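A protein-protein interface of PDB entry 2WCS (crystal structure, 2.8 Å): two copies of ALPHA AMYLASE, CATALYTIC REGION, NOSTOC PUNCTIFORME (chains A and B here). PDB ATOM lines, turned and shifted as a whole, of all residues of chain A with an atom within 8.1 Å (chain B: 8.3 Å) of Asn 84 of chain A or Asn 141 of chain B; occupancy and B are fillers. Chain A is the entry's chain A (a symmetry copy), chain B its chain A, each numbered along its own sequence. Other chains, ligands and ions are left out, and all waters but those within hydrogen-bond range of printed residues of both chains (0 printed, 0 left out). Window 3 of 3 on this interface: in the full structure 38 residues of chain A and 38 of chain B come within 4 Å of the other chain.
Of the 17 printed residues of chain B, 7 touch a printed residue of chain A. Printed residues of chain B that touch a printed residue of chain A: His 136, Asp 137, Leu 139, Glu 140, Asn 141, Pro 146 and Trp 147. Hydrophobic or aromatic side chains of chain B that line the printed part of chain A: His 136, Leu 139, Pro 146 and Trp 147. Of the 16 printed residues of chain A, 7 touch a printed residue of chain B. Hydrophobic or aromatic side chains of chain A within 4 Å of the printed part of chain B: Ala 82, His 85, Met 98 and Tyr 161. Among the printed residues, 13 pairs touch across the chains. Among the printed residues, Asp or Glu carboxylates within 4 Å of a Lys or Arg side-chain nitrogen of the other chain: Arg 130 of chain A with Glu 140 of chain B (3.0 Å).
No position is printed for both chains.
OD1 of Asn 141 of chain B lies close to OD1 of Asp 137 of chain B. The side-chain hydroxyl (OG) of Ser 145 of chain B lies within hydrogen-bond range of the side-chain carboxylate (OD1) of Asp 137 of chain B (2.6 Å). O of Ser 83 of chain A lies within hydrogen-bond range of ND1 of His 85 of chain A, 2.7 Å away. The side-chain carboxylate (OD1) of Asp 96 of chain A sits at hydrogen-bond distance from the backbone NH (N) of Met 98 of chain A (2.8 Å).
Of chain B, only Asp 137, Asn 141 and Pro 146 come within 4 Å of Ser 83 of chain A. Of the printed residues of chain B, Asn 84 of chain A touches Asn 141. Of the printed residues of chain B, His 85 of chain A touches Asn 141. Arg 86 of chain A touches none of the printed residues of chain B. Printed residues of chain A within 4 Å of Glu 140 of chain B: Ala 82, Arg 130 and Tyr 161. No residue of chain A comes within 4 Å of Gly 142 of chain B. Ser 145 of chain B touches none of the printed residues of chain A. Of the printed residues of chain A, Pro 146 of chain B touches Ser 83 (3.4 Å). Of the printed residues of chain A, Trp 147 of chain B touches Met 98. The nearest residue of chain B that does not touch Asn 84 of chain A is His 144 of chain B (6.2 Å). The nearest residue of chain A that does not touch Asn 141 of chain B is Ala 82 of chain A (4.5 Å). The nearest printed residue of chain A that does not touch Asp 137 of chain B is Ser 81 of chain A (4.6 Å).
Ala 82 of chain A touches Asp 137 of chain B (CA to OD2, 3.5 Å). Ala 82 of chain A touches Glu 140 of chain B. Ser 83 of chain A touches Pro 146 of chain B (OG to CG, 3.4 Å). Asn 84 of chain A touches Asn 141 of chain B. SD of Met 98 of chain A touches CZ2 of Trp 147 of chain B (3.5 Å). Arg 130 of chain A touches His 136 of chain B. ND1 of His 136 of chain B touches OH of Tyr 161 of chain A, 3.96 Å away. Leu 139 of chain B touches Tyr 161 of chain A (O to CE2, 3.4 Å).
The side-chain amide nitrogen (ND2) of Asn 141 of chain B sits close to a ring nitrogen (ND1) of His 85 of chain A (3.4 Å). OE1 of Glu 140 of chain B is in hydrogen-bond range of OH of Tyr 161 of chain A, at 2.8 Å. OD2 of Asp 137 of chain B lies within hydrogen-bond range of N of Ser 83 of chain A (3.0 Å). OD1 of Asn 141 of chain B lies close to O of Ser 83 of chain A. The side-chain carboxylate of Glu 140 of chain B lies within salt-bridge range of the guanidinium group of Arg 130 of chain A, 3.0 Å away.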
ATOM      1  N   PHE A  18     -28.219  25.095 -28.750  1.00  0.00           N
ATOM      2  CA  PHE A  18     -28.289  23.690 -28.369  1.00  0.00           C
ATOM      3  C   PHE A  18     -27.804  22.787 -29.498  1.00  0.00           C
ATOM      4  O   PHE A  18     -28.579  22.393 -30.368  1.00  0.00           O
ATOM      5  CB  PHE A  18     -29.718  23.312 -27.971  1.00  0.00           C
ATOM      6  CG  PHE A  18     -29.838  21.941 -27.374  1.00  0.00           C
ATOM      7  CD1 PHE A  18     -29.742  20.812 -28.170  1.00  0.00           C
ATOM      8  CD2 PHE A  18     -30.047  21.779 -26.014  1.00  0.00           C
ATOM      9  CE1 PHE A  18     -29.853  19.548 -27.622  1.00  0.00           C
ATOM     10  CE2 PHE A  18     -30.159  20.517 -25.460  1.00  0.00           C
ATOM     11  CZ  PHE A  18     -30.062  19.400 -26.267  1.00  0.00           C
ATOM     12  N   ASP A  20     -27.024  19.919 -30.399  1.00  0.00           N
ATOM     13  CA  ASP A  20     -27.596  18.648 -30.825  1.00  0.00           C
ATOM     14  C   ASP A  20     -28.850  18.862 -31.669  1.00  0.00           C
ATOM     15  O   ASP A  20     -29.259  17.981 -32.423  1.00  0.00           O
ATOM     16  CB  ASP A  20     -27.924  17.775 -29.611  1.00  0.00           C
ATOM     17  CG  ASP A  20     -26.960  16.618 -29.448  1.00  0.00           C
ATOM     18  OD1 ASP A  20     -26.864  16.074 -28.327  1.00  0.00           O
ATOM     19  OD2 ASP A  20     -26.295  16.252 -30.440  1.00  0.00           O
ATOM     20  N   ARG A  21     -29.450  20.041 -31.537  1.00  0.00           N
ATOM     21  CA  ARG A  21     -30.672  20.359 -32.261  1.00  0.00           C
ATOM     22  C   ARG A  21     -30.623  21.662 -33.040  1.00  0.00           C
ATOM     23  O   ARG A  21     -31.659  22.195 -33.416  1.00  0.00           O
ATOM     24  CB  ARG A  21     -31.855  20.390 -31.289  1.00  0.00           C
ATOM     25  CG  ARG A  21     -32.319  19.013 -30.845  1.00  0.00           C
ATOM     26  CD  ARG A  21     -32.969  18.258 -32.000  1.00  0.00           C
ATOM     27  NE  ARG A  21     -33.284  16.873 -31.662  1.00  0.00           N
ATOM     28  CZ  ARG A  21     -32.376  15.912 -31.508  1.00  0.00           C
ATOM     29  NH1 ARG A  21     -31.086  16.178 -31.662  1.00  0.00           N
ATOM     30  NH2 ARG A  21     -32.758  14.679 -31.199  1.00  0.00           N
ATOM     31  N   SER A  81     -20.984  12.219 -23.486  1.00  0.00           N
ATOM     32  CA  SER A  81     -22.041  11.806 -22.575  1.00  0.00           C
ATOM     33  C   SER A  81     -22.997  10.947 -23.384  1.00  0.00           C
ATOM     34  O   SER A  81     -22.912  10.925 -24.607  1.00  0.00           O
ATOM     35  CB  SER A  81     -22.790  13.029 -22.046  1.00  0.00           C
ATOM     36  OG  SER A  81     -23.328  13.782 -23.119  1.00  0.00           O
ATOM     37  N   ALA A  82     -23.905  10.244 -22.718  1.00  0.00           N
ATOM     38  CA  ALA A  82     -24.852   9.409 -23.442  1.00  0.00           C
ATOM     39  C   ALA A  82     -25.819  10.307 -24.203  1.00  0.00           C
ATOM     40  O   ALA A  82     -26.029  11.462 -23.822  1.00  0.00           O
ATOM     41  CB  ALA A  82     -25.612   8.507 -22.478  1.00  0.00           C
ATOM     42  N   SER A  83     -26.389   9.779 -25.285  1.00  0.00           N
ATOM     43  CA  SER A  83     -27.333  10.527 -26.106  1.00  0.00           C
ATOM     44  C   SER A  83     -28.367  11.229 -25.240  1.00  0.00           C
ATOM     45  O   SER A  83     -28.783  10.695 -24.211  1.00  0.00           O
ATOM     46  CB  SER A  83     -28.039   9.591 -27.080  1.00  0.00           C
ATOM     47  OG  SER A  83     -27.107   8.972 -27.942  1.00  0.00           O
ATOM     48  N   ASN A  84     -28.774  12.423 -25.672  1.00  0.00           N
ATOM     49  CA  ASN A  84     -29.754  13.246 -24.967  1.00  0.00           C
ATOM     50  C   ASN A  84     -29.632  13.180 -23.445  1.00  0.00           C
ATOM     51  O   ASN A  84     -30.626  13.071 -22.724  1.00  0.00           O
ATOM     52  CB  ASN A  84     -31.183  12.884 -25.400  1.00  0.00           C
ATOM     53  CG  ASN A  84     -31.558  11.453 -25.068  1.00  0.00           C
ATOM     54  OD1 ASN A  84     -31.002  10.505 -25.623  1.00  0.00           O
ATOM     55  ND2 ASN A  84     -32.511  11.290 -24.159  1.00  0.00           N
ATOM     56  N   HIS A  85     -28.393  13.249 -22.970  1.00  0.00           N
ATOM     57  CA  HIS A  85     -28.081  13.229 -21.550  1.00  0.00           C
ATOM     58  C   HIS A  85     -26.793  14.028 -21.375  1.00  0.00           C
ATOM     59  O   HIS A  85     -25.995  13.736 -20.484  1.00  0.00           O
ATOM     60  CB  HIS A  85     -27.855  11.798 -21.060  1.00  0.00           C
ATOM     61  CG  HIS A  85     -29.116  11.047 -20.767  1.00  0.00           C
ATOM     62  ND1 HIS A  85     -29.978  10.621 -21.753  1.00  0.00           N
ATOM     63  CD2 HIS A  85     -29.656  10.641 -19.594  1.00  0.00           C
ATOM     64  CE1 HIS A  85     -30.995   9.985 -21.200  1.00  0.00           C
ATOM     65  NE2 HIS A  85     -30.824   9.982 -19.892  1.00  0.00           N
ATOM     66  N   ARG A  86     -26.612  15.031 -22.236  1.00  0.00           N
ATOM     67  CA  ARG A  86     -25.426  15.889 -22.246  1.00  0.00           C
ATOM     68  C   ARG A  86     -24.930  16.378 -20.878  1.00  0.00           C
ATOM     69  O   ARG A  86     -23.778  16.802 -20.753  1.00  0.00           O
ATOM     70  CB  ARG A  86     -25.667  17.108 -23.139  1.00  0.00           C
ATOM     71  CG  ARG A  86     -26.247  16.824 -24.518  1.00  0.00           C
ATOM     72  CD  ARG A  86     -25.198  16.526 -25.571  1.00  0.00           C
ATOM     73  NE  ARG A  86     -24.756  15.139 -25.527  1.00  0.00           N
ATOM     74  CZ  ARG A  86     -24.405  14.432 -26.596  1.00  0.00           C
ATOM     75  NH1 ARG A  86     -24.441  14.977 -27.804  1.00  0.00           N
ATOM     76  NH2 ARG A  86     -24.021  13.175 -26.454  1.00  0.00           N
ATOM     77  N   TYR A  87     -25.785  16.332 -19.861  1.00  0.00           N
ATOM     78  CA  TYR A  87     -25.401  16.774 -18.518  1.00  0.00           C
ATOM     79  C   TYR A  87     -24.817  15.641 -17.676  1.00  0.00           C
ATOM     80  O   TYR A  87     -24.316  15.867 -16.576  1.00  0.00           O
ATOM     81  CB  TYR A  87     -26.607  17.399 -17.805  1.00  0.00           C
ATOM     82  CG  TYR A  87     -26.903  18.808 -18.259  1.00  0.00           C
ATOM     83  CD1 TYR A  87     -26.207  19.892 -17.726  1.00  0.00           C
ATOM     84  CD2 TYR A  87     -27.843  19.056 -19.255  1.00  0.00           C
ATOM     85  CE1 TYR A  87     -26.439  21.190 -18.176  1.00  0.00           C
ATOM     86  CE2 TYR A  87     -28.083  20.345 -19.714  1.00  0.00           C
ATOM     87  CZ  TYR A  87     -27.379  21.407 -19.172  1.00  0.00           C
ATOM     88  OH  TYR A  87     -27.605  22.679 -19.639  1.00  0.00           O
ATOM     89  N   HIS A  88     -24.899  14.423 -18.196  1.00  0.00           N
ATOM     90  CA  HIS A  88     -24.354  13.254 -17.516  1.00  0.00           C
ATOM     91  C   HIS A  88     -22.975  13.033 -18.126  1.00  0.00           C
ATOM     92  O   HIS A  88     -22.752  12.055 -18.837  1.00  0.00           O
ATOM     93  CB  HIS A  88     -25.226  12.032 -17.784  1.00  0.00           C
ATOM     94  CG  HIS A  88     -26.633  12.165 -17.294  1.00  0.00           C
ATOM     95  ND1 HIS A  88     -27.020  11.793 -16.024  1.00  0.00           N
ATOM     96  CD2 HIS A  88     -27.756  12.594 -17.917  1.00  0.00           C
ATOM     97  CE1 HIS A  88     -28.321  11.981 -15.890  1.00  0.00           C
ATOM     98  NE2 HIS A  88     -28.792  12.466 -17.024  1.00  0.00           N
ATOM     99  N   ASP A  96     -18.258  15.247 -27.623  1.00  0.00           N
ATOM    100  CA  ASP A  96     -19.036  14.069 -27.985  1.00  0.00           C
ATOM    101  C   ASP A  96     -18.855  13.720 -29.458  1.00  0.00           C
ATOM    102  O   ASP A  96     -18.977  14.580 -30.331  1.00  0.00           O
ATOM    103  CB  ASP A  96     -20.518  14.289 -27.675  1.00  0.00           C
ATOM    104  CG  ASP A  96     -21.327  13.010 -27.759  1.00  0.00           C
ATOM    105  OD1 ASP A  96     -21.642  12.576 -28.887  1.00  0.00           O
ATOM    106  OD2 ASP A  96     -21.649  12.438 -26.696  1.00  0.00           O
ATOM    107  N   MET A  98     -20.707  12.219 -31.512  1.00  0.00           N
ATOM    108  CA  MET A  98     -21.900  12.443 -32.319  1.00  0.00           C
ATOM    109  C   MET A  98     -22.011  13.903 -32.744  1.00  0.00           C
ATOM    110  O   MET A  98     -22.748  14.235 -33.673  1.00  0.00           O
ATOM    111  CB  MET A  98     -23.153  12.024 -31.548  1.00  0.00           C
ATOM    112  CG  MET A  98     -23.195  10.548 -31.187  1.00  0.00           C
ATOM    113  SD  MET A  98     -23.059   9.474 -32.629  1.00  0.00           S
ATOM    114  CE  MET A  98     -21.279   9.364 -32.801  1.00  0.00           C
ATOM    115  N   ARG A 130     -22.637   7.938 -14.389  1.00  0.00           N
ATOM    116  CA  ARG A 130     -22.199   6.618 -13.948  1.00  0.00           C
ATOM    117  C   ARG A 130     -20.980   6.135 -14.743  1.00  0.00           C
ATOM    118  O   ARG A 130     -20.130   5.421 -14.212  1.00  0.00           O
ATOM    119  CB  ARG A 130     -23.335   5.609 -14.108  1.00  0.00           C
ATOM    120  CG  ARG A 130     -24.576   5.885 -13.279  1.00  0.00           C
ATOM    121  CD  ARG A 130     -25.794   5.921 -14.181  1.00  0.00           C
ATOM    122  NE  ARG A 130     -27.007   5.479 -13.505  1.00  0.00           N
ATOM    123  CZ  ARG A 130     -28.213   5.483 -14.064  1.00  0.00           C
ATOM    124  NH1 ARG A 130     -28.367   5.915 -15.308  1.00  0.00           N
ATOM    125  NH2 ARG A 130     -29.264   5.042 -13.385  1.00  0.00           N
ATOM    126  N   TYR A 161     -28.207   1.460 -10.962  1.00  0.00           N
ATOM    127  CA  TYR A 161     -29.187   1.346 -12.038  1.00  0.00           C
ATOM    128  C   TYR A 161     -30.542   0.754 -11.664  1.00  0.00           C
ATOM    129  O   TYR A 161     -31.570   1.155 -12.217  1.00  0.00           O
ATOM    130  CB  TYR A 161     -28.612   0.526 -13.197  1.00  0.00           C
ATOM    131  CG  TYR A 161     -27.587   1.248 -14.035  1.00  0.00           C
ATOM    132  CD1 TYR A 161     -26.232   1.208 -13.711  1.00  0.00           C
ATOM    133  CD2 TYR A 161     -27.975   1.973 -15.163  1.00  0.00           C
ATOM    134  CE1 TYR A 161     -25.290   1.869 -14.490  1.00  0.00           C
ATOM    135  CE2 TYR A 161     -27.043   2.638 -15.945  1.00  0.00           C
ATOM    136  CZ  TYR A 161     -25.704   2.584 -15.605  1.00  0.00           C
ATOM    137  OH  TYR A 161     -24.782   3.250 -16.380  1.00  0.00           O
ATOM    138  N   ASP A 369     -39.390  17.480 -25.518  1.00  0.00           N
ATOM    139  CA  ASP A 369     -39.525  17.356 -26.963  1.00  0.00           C
ATOM    140  C   ASP A 369     -40.890  17.849 -27.433  1.00  0.00           C
ATOM    141  O   ASP A 369     -41.431  17.355 -28.423  1.00  0.00           O
ATOM    142  CB  ASP A 369     -39.311  15.906 -27.400  1.00  0.00           C
ATOM    143  CG  ASP A 369     -37.856  15.485 -27.330  1.00  0.00           C
ATOM    144  OD1 ASP A 369     -37.052  15.982 -28.146  1.00  0.00           O
ATOM    145  OD2 ASP A 369     -37.517  14.656 -26.459  1.00  0.00           O
ATOM    146  N   PHE B 134     -19.806   3.454 -25.269  1.00  0.00           N
ATOM    147  CA  PHE B 134     -20.962   2.934 -25.990  1.00  0.00           C
ATOM    148  C   PHE B 134     -21.815   1.935 -25.221  1.00  0.00           C
ATOM    149  O   PHE B 134     -23.032   1.889 -25.396  1.00  0.00           O
ATOM    150  CB  PHE B 134     -20.514   2.352 -27.321  1.00  0.00           C
ATOM    151  CG  PHE B 134     -19.688   3.303 -28.122  1.00  0.00           C
ATOM    152  CD1 PHE B 134     -18.321   3.429 -27.883  1.00  0.00           C
ATOM    153  CD2 PHE B 134     -20.282   4.132 -29.071  1.00  0.00           C
ATOM    154  CE1 PHE B 134     -17.562   4.364 -28.575  1.00  0.00           C
ATOM    155  CE2 PHE B 134     -19.521   5.077 -29.766  1.00  0.00           C
ATOM    156  CZ  PHE B 134     -18.164   5.192 -29.518  1.00  0.00           C
ATOM    157  N   PHE B 135     -21.199   1.131 -24.371  1.00  0.00           N
ATOM    158  CA  PHE B 135     -21.991   0.203 -23.597  1.00  0.00           C
ATOM    159  C   PHE B 135     -22.793   1.099 -22.651  1.00  0.00           C
ATOM    160  O   PHE B 135     -24.014   0.971 -22.534  1.00  0.00           O
ATOM    161  CB  PHE B 135     -21.102  -0.755 -22.803  1.00  0.00           C
ATOM    162  CG  PHE B 135     -21.862  -1.872 -22.152  1.00  0.00           C
ATOM    163  CD1 PHE B 135     -22.640  -2.739 -22.921  1.00  0.00           C
ATOM    164  CD2 PHE B 135     -21.840  -2.038 -20.771  1.00  0.00           C
ATOM    165  CE1 PHE B 135     -23.389  -3.754 -22.322  1.00  0.00           C
ATOM    166  CE2 PHE B 135     -22.584  -3.051 -20.162  1.00  0.00           C
ATOM    167  CZ  PHE B 135     -23.361  -3.909 -20.940  1.00  0.00           C
ATOM    168  N   HIS B 136     -22.080   2.012 -21.992  1.00  0.00           N
ATOM    169  CA  HIS B 136     -22.665   2.978 -21.068  1.00  0.00           C
ATOM    170  C   HIS B 136     -23.903   3.630 -21.697  1.00  0.00           C
ATOM    171  O   HIS B 136     -24.971   3.680 -21.088  1.00  0.00           O
ATOM    172  CB  HIS B 136     -21.620   4.052 -20.752  1.00  0.00           C
ATOM    173  CG  HIS B 136     -22.161   5.241 -20.017  1.00  0.00           C
ATOM    174  ND1 HIS B 136     -22.259   5.291 -18.644  1.00  0.00           N
ATOM    175  CD2 HIS B 136     -22.635   6.425 -20.471  1.00  0.00           C
ATOM    176  CE1 HIS B 136     -22.770   6.454 -18.283  1.00  0.00           C
ATOM    177  NE2 HIS B 136     -23.007   7.160 -19.372  1.00  0.00           N
ATOM    178  N   ASP B 137     -23.750   4.131 -22.919  1.00  0.00           N
ATOM    179  CA  ASP B 137     -24.858   4.777 -23.603  1.00  0.00           C
ATOM    180  C   ASP B 137     -26.038   3.824 -23.644  1.00  0.00           C
ATOM    181  O   ASP B 137     -27.189   4.227 -23.478  1.00  0.00           O
ATOM    182  CB  ASP B 137     -24.460   5.168 -25.025  1.00  0.00           C
ATOM    183  CG  ASP B 137     -25.517   6.011 -25.714  1.00  0.00           C
ATOM    184  OD1 ASP B 137     -26.647   5.516 -25.906  1.00  0.00           O
ATOM    185  OD2 ASP B 137     -25.216   7.172 -26.065  1.00  0.00           O
ATOM    186  N   VAL B 138     -25.745   2.548 -23.859  1.00  0.00           N
ATOM    187  CA  VAL B 138     -26.793   1.546 -23.913  1.00  0.00           C
ATOM    188  C   VAL B 138     -27.411   1.362 -22.536  1.00  0.00           C
ATOM    189  O   VAL B 138     -28.621   1.213 -22.415  1.00  0.00           O
ATOM    190  CB  VAL B 138     -26.246   0.210 -24.423  1.00  0.00           C
ATOM    191  CG1 VAL B 138     -27.302  -0.868 -24.289  1.00  0.00           C
ATOM    192  CG2 VAL B 138     -25.825   0.356 -25.873  1.00  0.00           C
ATOM    193  N   LEU B 139     -26.580   1.384 -21.501  1.00  0.00           N
ATOM    194  CA  LEU B 139     -27.065   1.233 -20.135  1.00  0.00           C
ATOM    195  C   LEU B 139     -27.836   2.466 -19.687  1.00  0.00           C
ATOM    196  O   LEU B 139     -28.744   2.377 -18.863  1.00  0.00           O
ATOM    197  CB  LEU B 139     -25.903   1.011 -19.173  1.00  0.00           C
ATOM    198  CG  LEU B 139     -25.082  -0.256 -19.376  1.00  0.00           C
ATOM    199  CD1 LEU B 139     -24.103  -0.402 -18.212  1.00  0.00           C
ATOM    200  CD2 LEU B 139     -26.004  -1.471 -19.457  1.00  0.00           C
ATOM    201  N   GLU B 140     -27.465   3.618 -20.232  1.00  0.00           N
ATOM    202  CA  GLU B 140     -28.109   4.868 -19.870  1.00  0.00           C
ATOM    203  C   GLU B 140     -29.342   5.157 -20.725  1.00  0.00           C
ATOM    204  O   GLU B 140     -30.192   5.954 -20.337  1.00  0.00           O
ATOM    205  CB  GLU B 140     -27.110   6.023 -20.004  1.00  0.00           C
ATOM    206  CG  GLU B 140     -27.162   7.028 -18.863  1.00  0.00           C
ATOM    207  CD  GLU B 140     -26.412   6.551 -17.640  1.00  0.00           C
ATOM    208  OE1 GLU B 140     -26.321   5.322 -17.448  1.00  0.00           O
ATOM    209  OE2 GLU B 140     -25.922   7.404 -16.868  1.00  0.00           O
ATOM    210  N   ASN B 141     -29.447   4.506 -21.880  1.00  0.00           N
ATOM    211  CA  ASN B 141     -30.580   4.733 -22.779  1.00  0.00           C
ATOM    212  C   ASN B 141     -31.428   3.504 -23.089  1.00  0.00           C
ATOM    213  O   ASN B 141     -32.369   3.584 -23.884  1.00  0.00           O
ATOM    214  CB  ASN B 141     -30.090   5.334 -24.103  1.00  0.00           C
ATOM    215  CG  ASN B 141     -29.813   6.819 -24.004  1.00  0.00           C
ATOM    216  OD1 ASN B 141     -29.247   7.418 -24.919  1.00  0.00           O
ATOM    217  ND2 ASN B 141     -30.217   7.424 -22.894  1.00  0.00           N
ATOM    218  N   GLY B 142     -31.097   2.373 -22.475  1.00  0.00           N
ATOM    219  CA  GLY B 142     -31.854   1.159 -22.729  1.00  0.00           C
ATOM    220  C   GLY B 142     -32.191   0.944 -24.197  1.00  0.00           C
ATOM    221  O   GLY B 142     -31.375   1.223 -25.074  1.00  0.00           O
ATOM    222  N   PRO B 143     -33.400   0.455 -24.503  1.00  0.00           N
ATOM    223  CA  PRO B 143     -33.833   0.202 -25.879  1.00  0.00           C
ATOM    224  C   PRO B 143     -33.607   1.354 -26.845  1.00  0.00           C
ATOM    225  O   PRO B 143     -33.263   1.140 -28.007  1.00  0.00           O
ATOM    226  CB  PRO B 143     -35.313  -0.115 -25.713  1.00  0.00           C
ATOM    227  CG  PRO B 143     -35.345  -0.806 -24.395  1.00  0.00           C
ATOM    228  CD  PRO B 143     -34.453   0.070 -23.548  1.00  0.00           C
ATOM    229  N   HIS B 144     -33.795   2.576 -26.356  1.00  0.00           N
ATOM    230  CA  HIS B 144     -33.650   3.772 -27.181  1.00  0.00           C
ATOM    231  C   HIS B 144     -32.224   4.152 -27.555  1.00  0.00           C
ATOM    232  O   HIS B 144     -32.022   5.072 -28.343  1.00  0.00           O
ATOM    233  CB  HIS B 144     -34.321   4.958 -26.489  1.00  0.00           C
ATOM    234  CG  HIS B 144     -35.770   4.737 -26.186  1.00  0.00           C
ATOM    235  ND1 HIS B 144     -36.705   4.483 -27.167  1.00  0.00           N
ATOM    236  CD2 HIS B 144     -36.444   4.728 -25.012  1.00  0.00           C
ATOM    237  CE1 HIS B 144     -37.892   4.326 -26.609  1.00  0.00           C
ATOM    238  NE2 HIS B 144     -37.762   4.470 -25.303  1.00  0.00           N
ATOM    239  N   SER B 145     -31.236   3.456 -26.998  1.00  0.00           N
ATOM    240  CA  SER B 145     -29.838   3.757 -27.303  1.00  0.00           C
ATOM    241  C   SER B 145     -29.476   3.444 -28.758  1.00  0.00           C
ATOM    242  O   SER B 145     -29.939   2.456 -29.325  1.00  0.00           O
ATOM    243  CB  SER B 145     -28.913   2.987 -26.371  1.00  0.00           C
ATOM    244  OG  SER B 145     -27.567   3.269 -26.693  1.00  0.00           O
ATOM    245  N   PRO B 146     -28.624   4.281 -29.371  1.00  0.00           N
ATOM    246  CA  PRO B 146     -28.170   4.150 -30.761  1.00  0.00           C
ATOM    247  C   PRO B 146     -27.207   3.000 -31.053  1.00  0.00           C
ATOM    248  O   PRO B 146     -26.958   2.683 -32.217  1.00  0.00           O
ATOM    249  CB  PRO B 146     -27.499   5.500 -31.045  1.00  0.00           C
ATOM    250  CG  PRO B 146     -27.987   6.399 -29.957  1.00  0.00           C
ATOM    251  CD  PRO B 146     -28.057   5.494 -28.769  1.00  0.00           C
ATOM    252  N   TRP B 147     -26.659   2.383 -30.012  1.00  0.00           N
ATOM    253  CA  TRP B 147     -25.709   1.303 -30.229  1.00  0.00           C
ATOM    254  C   TRP B 147     -26.080  -0.033 -29.614  1.00  0.00           C
ATOM    255  O   TRP B 147     -25.211  -0.864 -29.352  1.00  0.00           O
ATOM    256  CB  TRP B 147     -24.334   1.732 -29.730  1.00  0.00           C
ATOM    257  CG  TRP B 147     -23.832   2.933 -30.443  1.00  0.00           C
ATOM    258  CD1 TRP B 147     -23.352   2.997 -31.724  1.00  0.00           C
ATOM    259  CD2 TRP B 147     -23.807   4.265 -29.939  1.00  0.00           C
ATOM    260  NE1 TRP B 147     -23.029   4.293 -32.045  1.00  0.00           N
ATOM    261  CE2 TRP B 147     -23.300   5.092 -30.966  1.00  0.00           C
ATOM    262  CE3 TRP B 147     -24.166   4.842 -28.717  1.00  0.00           C
ATOM    263  CZ2 TRP B 147     -23.144   6.466 -30.807  1.00  0.00           C
ATOM    264  CZ3 TRP B 147     -24.012   6.211 -28.560  1.00  0.00           C
ATOM    265  CH2 TRP B 147     -23.505   7.009 -29.599  1.00  0.00           C
ATOM    266  N   VAL B 148     -27.368  -0.241 -29.381  1.00  0.00           N
ATOM    267  CA  VAL B 148     -27.834  -1.495 -28.813  1.00  0.00           C
ATOM    268  C   VAL B 148     -27.300  -2.647 -29.675  1.00  0.00           C
ATOM    269  O   VAL B 148     -26.891  -3.688 -29.162  1.00  0.00           O
ATOM    270  CB  VAL B 148     -29.372  -1.539 -28.796  1.00  0.00           C
ATOM    271  CG1 VAL B 148     -29.851  -2.883 -28.283  1.00  0.00           C
ATOM    272  CG2 VAL B 148     -29.912  -0.412 -27.932  1.00  0.00           C
ATOM    273  N   TRP B 156     -34.567  -7.190 -22.239  1.00  0.00           N
ATOM    274  CA  TRP B 156     -34.621  -6.034 -21.354  1.00  0.00           C
ATOM    275  C   TRP B 156     -35.558  -6.304 -20.188  1.00  0.00           C
ATOM    276  O   TRP B 156     -36.525  -7.046 -20.324  1.00  0.00           O
ATOM    277  CB  TRP B 156     -35.099  -4.806 -22.130  1.00  0.00           C
ATOM    278  CG  TRP B 156     -34.039  -4.190 -23.000  1.00  0.00           C
ATOM    279  CD1 TRP B 156     -32.908  -3.533 -22.584  1.00  0.00           C
ATOM    280  CD2 TRP B 156     -34.018  -4.153 -24.432  1.00  0.00           C
ATOM    281  NE1 TRP B 156     -32.190  -3.089 -23.668  1.00  0.00           N
ATOM    282  CE2 TRP B 156     -32.847  -3.454 -24.815  1.00  0.00           C
ATOM    283  CE3 TRP B 156     -34.873  -4.642 -25.429  1.00  0.00           C
ATOM    284  CZ2 TRP B 156     -32.513  -3.232 -26.156  1.00  0.00           C
ATOM    285  CZ3 TRP B 156     -34.541  -4.420 -26.763  1.00  0.00           C
ATOM    286  CH2 TRP B 156     -33.368  -3.719 -27.113  1.00  0.00           C
ATOM    287  N   LEU B 158     -31.791  -4.746 -18.371  1.00  0.00           N
ATOM    288  CA  LEU B 158     -30.480  -5.279 -18.034  1.00  0.00           C
ATOM    289  C   LEU B 158     -30.096  -4.985 -16.592  1.00  0.00           C
ATOM    290  O   LEU B 158     -30.427  -3.925 -16.056  1.00  0.00           O
ATOM    291  CB  LEU B 158     -29.433  -4.673 -18.958  1.00  0.00           C
ATOM    292  CG  LEU B 158     -29.883  -4.570 -20.412  1.00  0.00           C
ATOM    293  CD1 LEU B 158     -28.772  -3.958 -21.251  1.00  0.00           C
ATOM    294  CD2 LEU B 158     -30.262  -5.948 -20.923  1.00  0.00           C
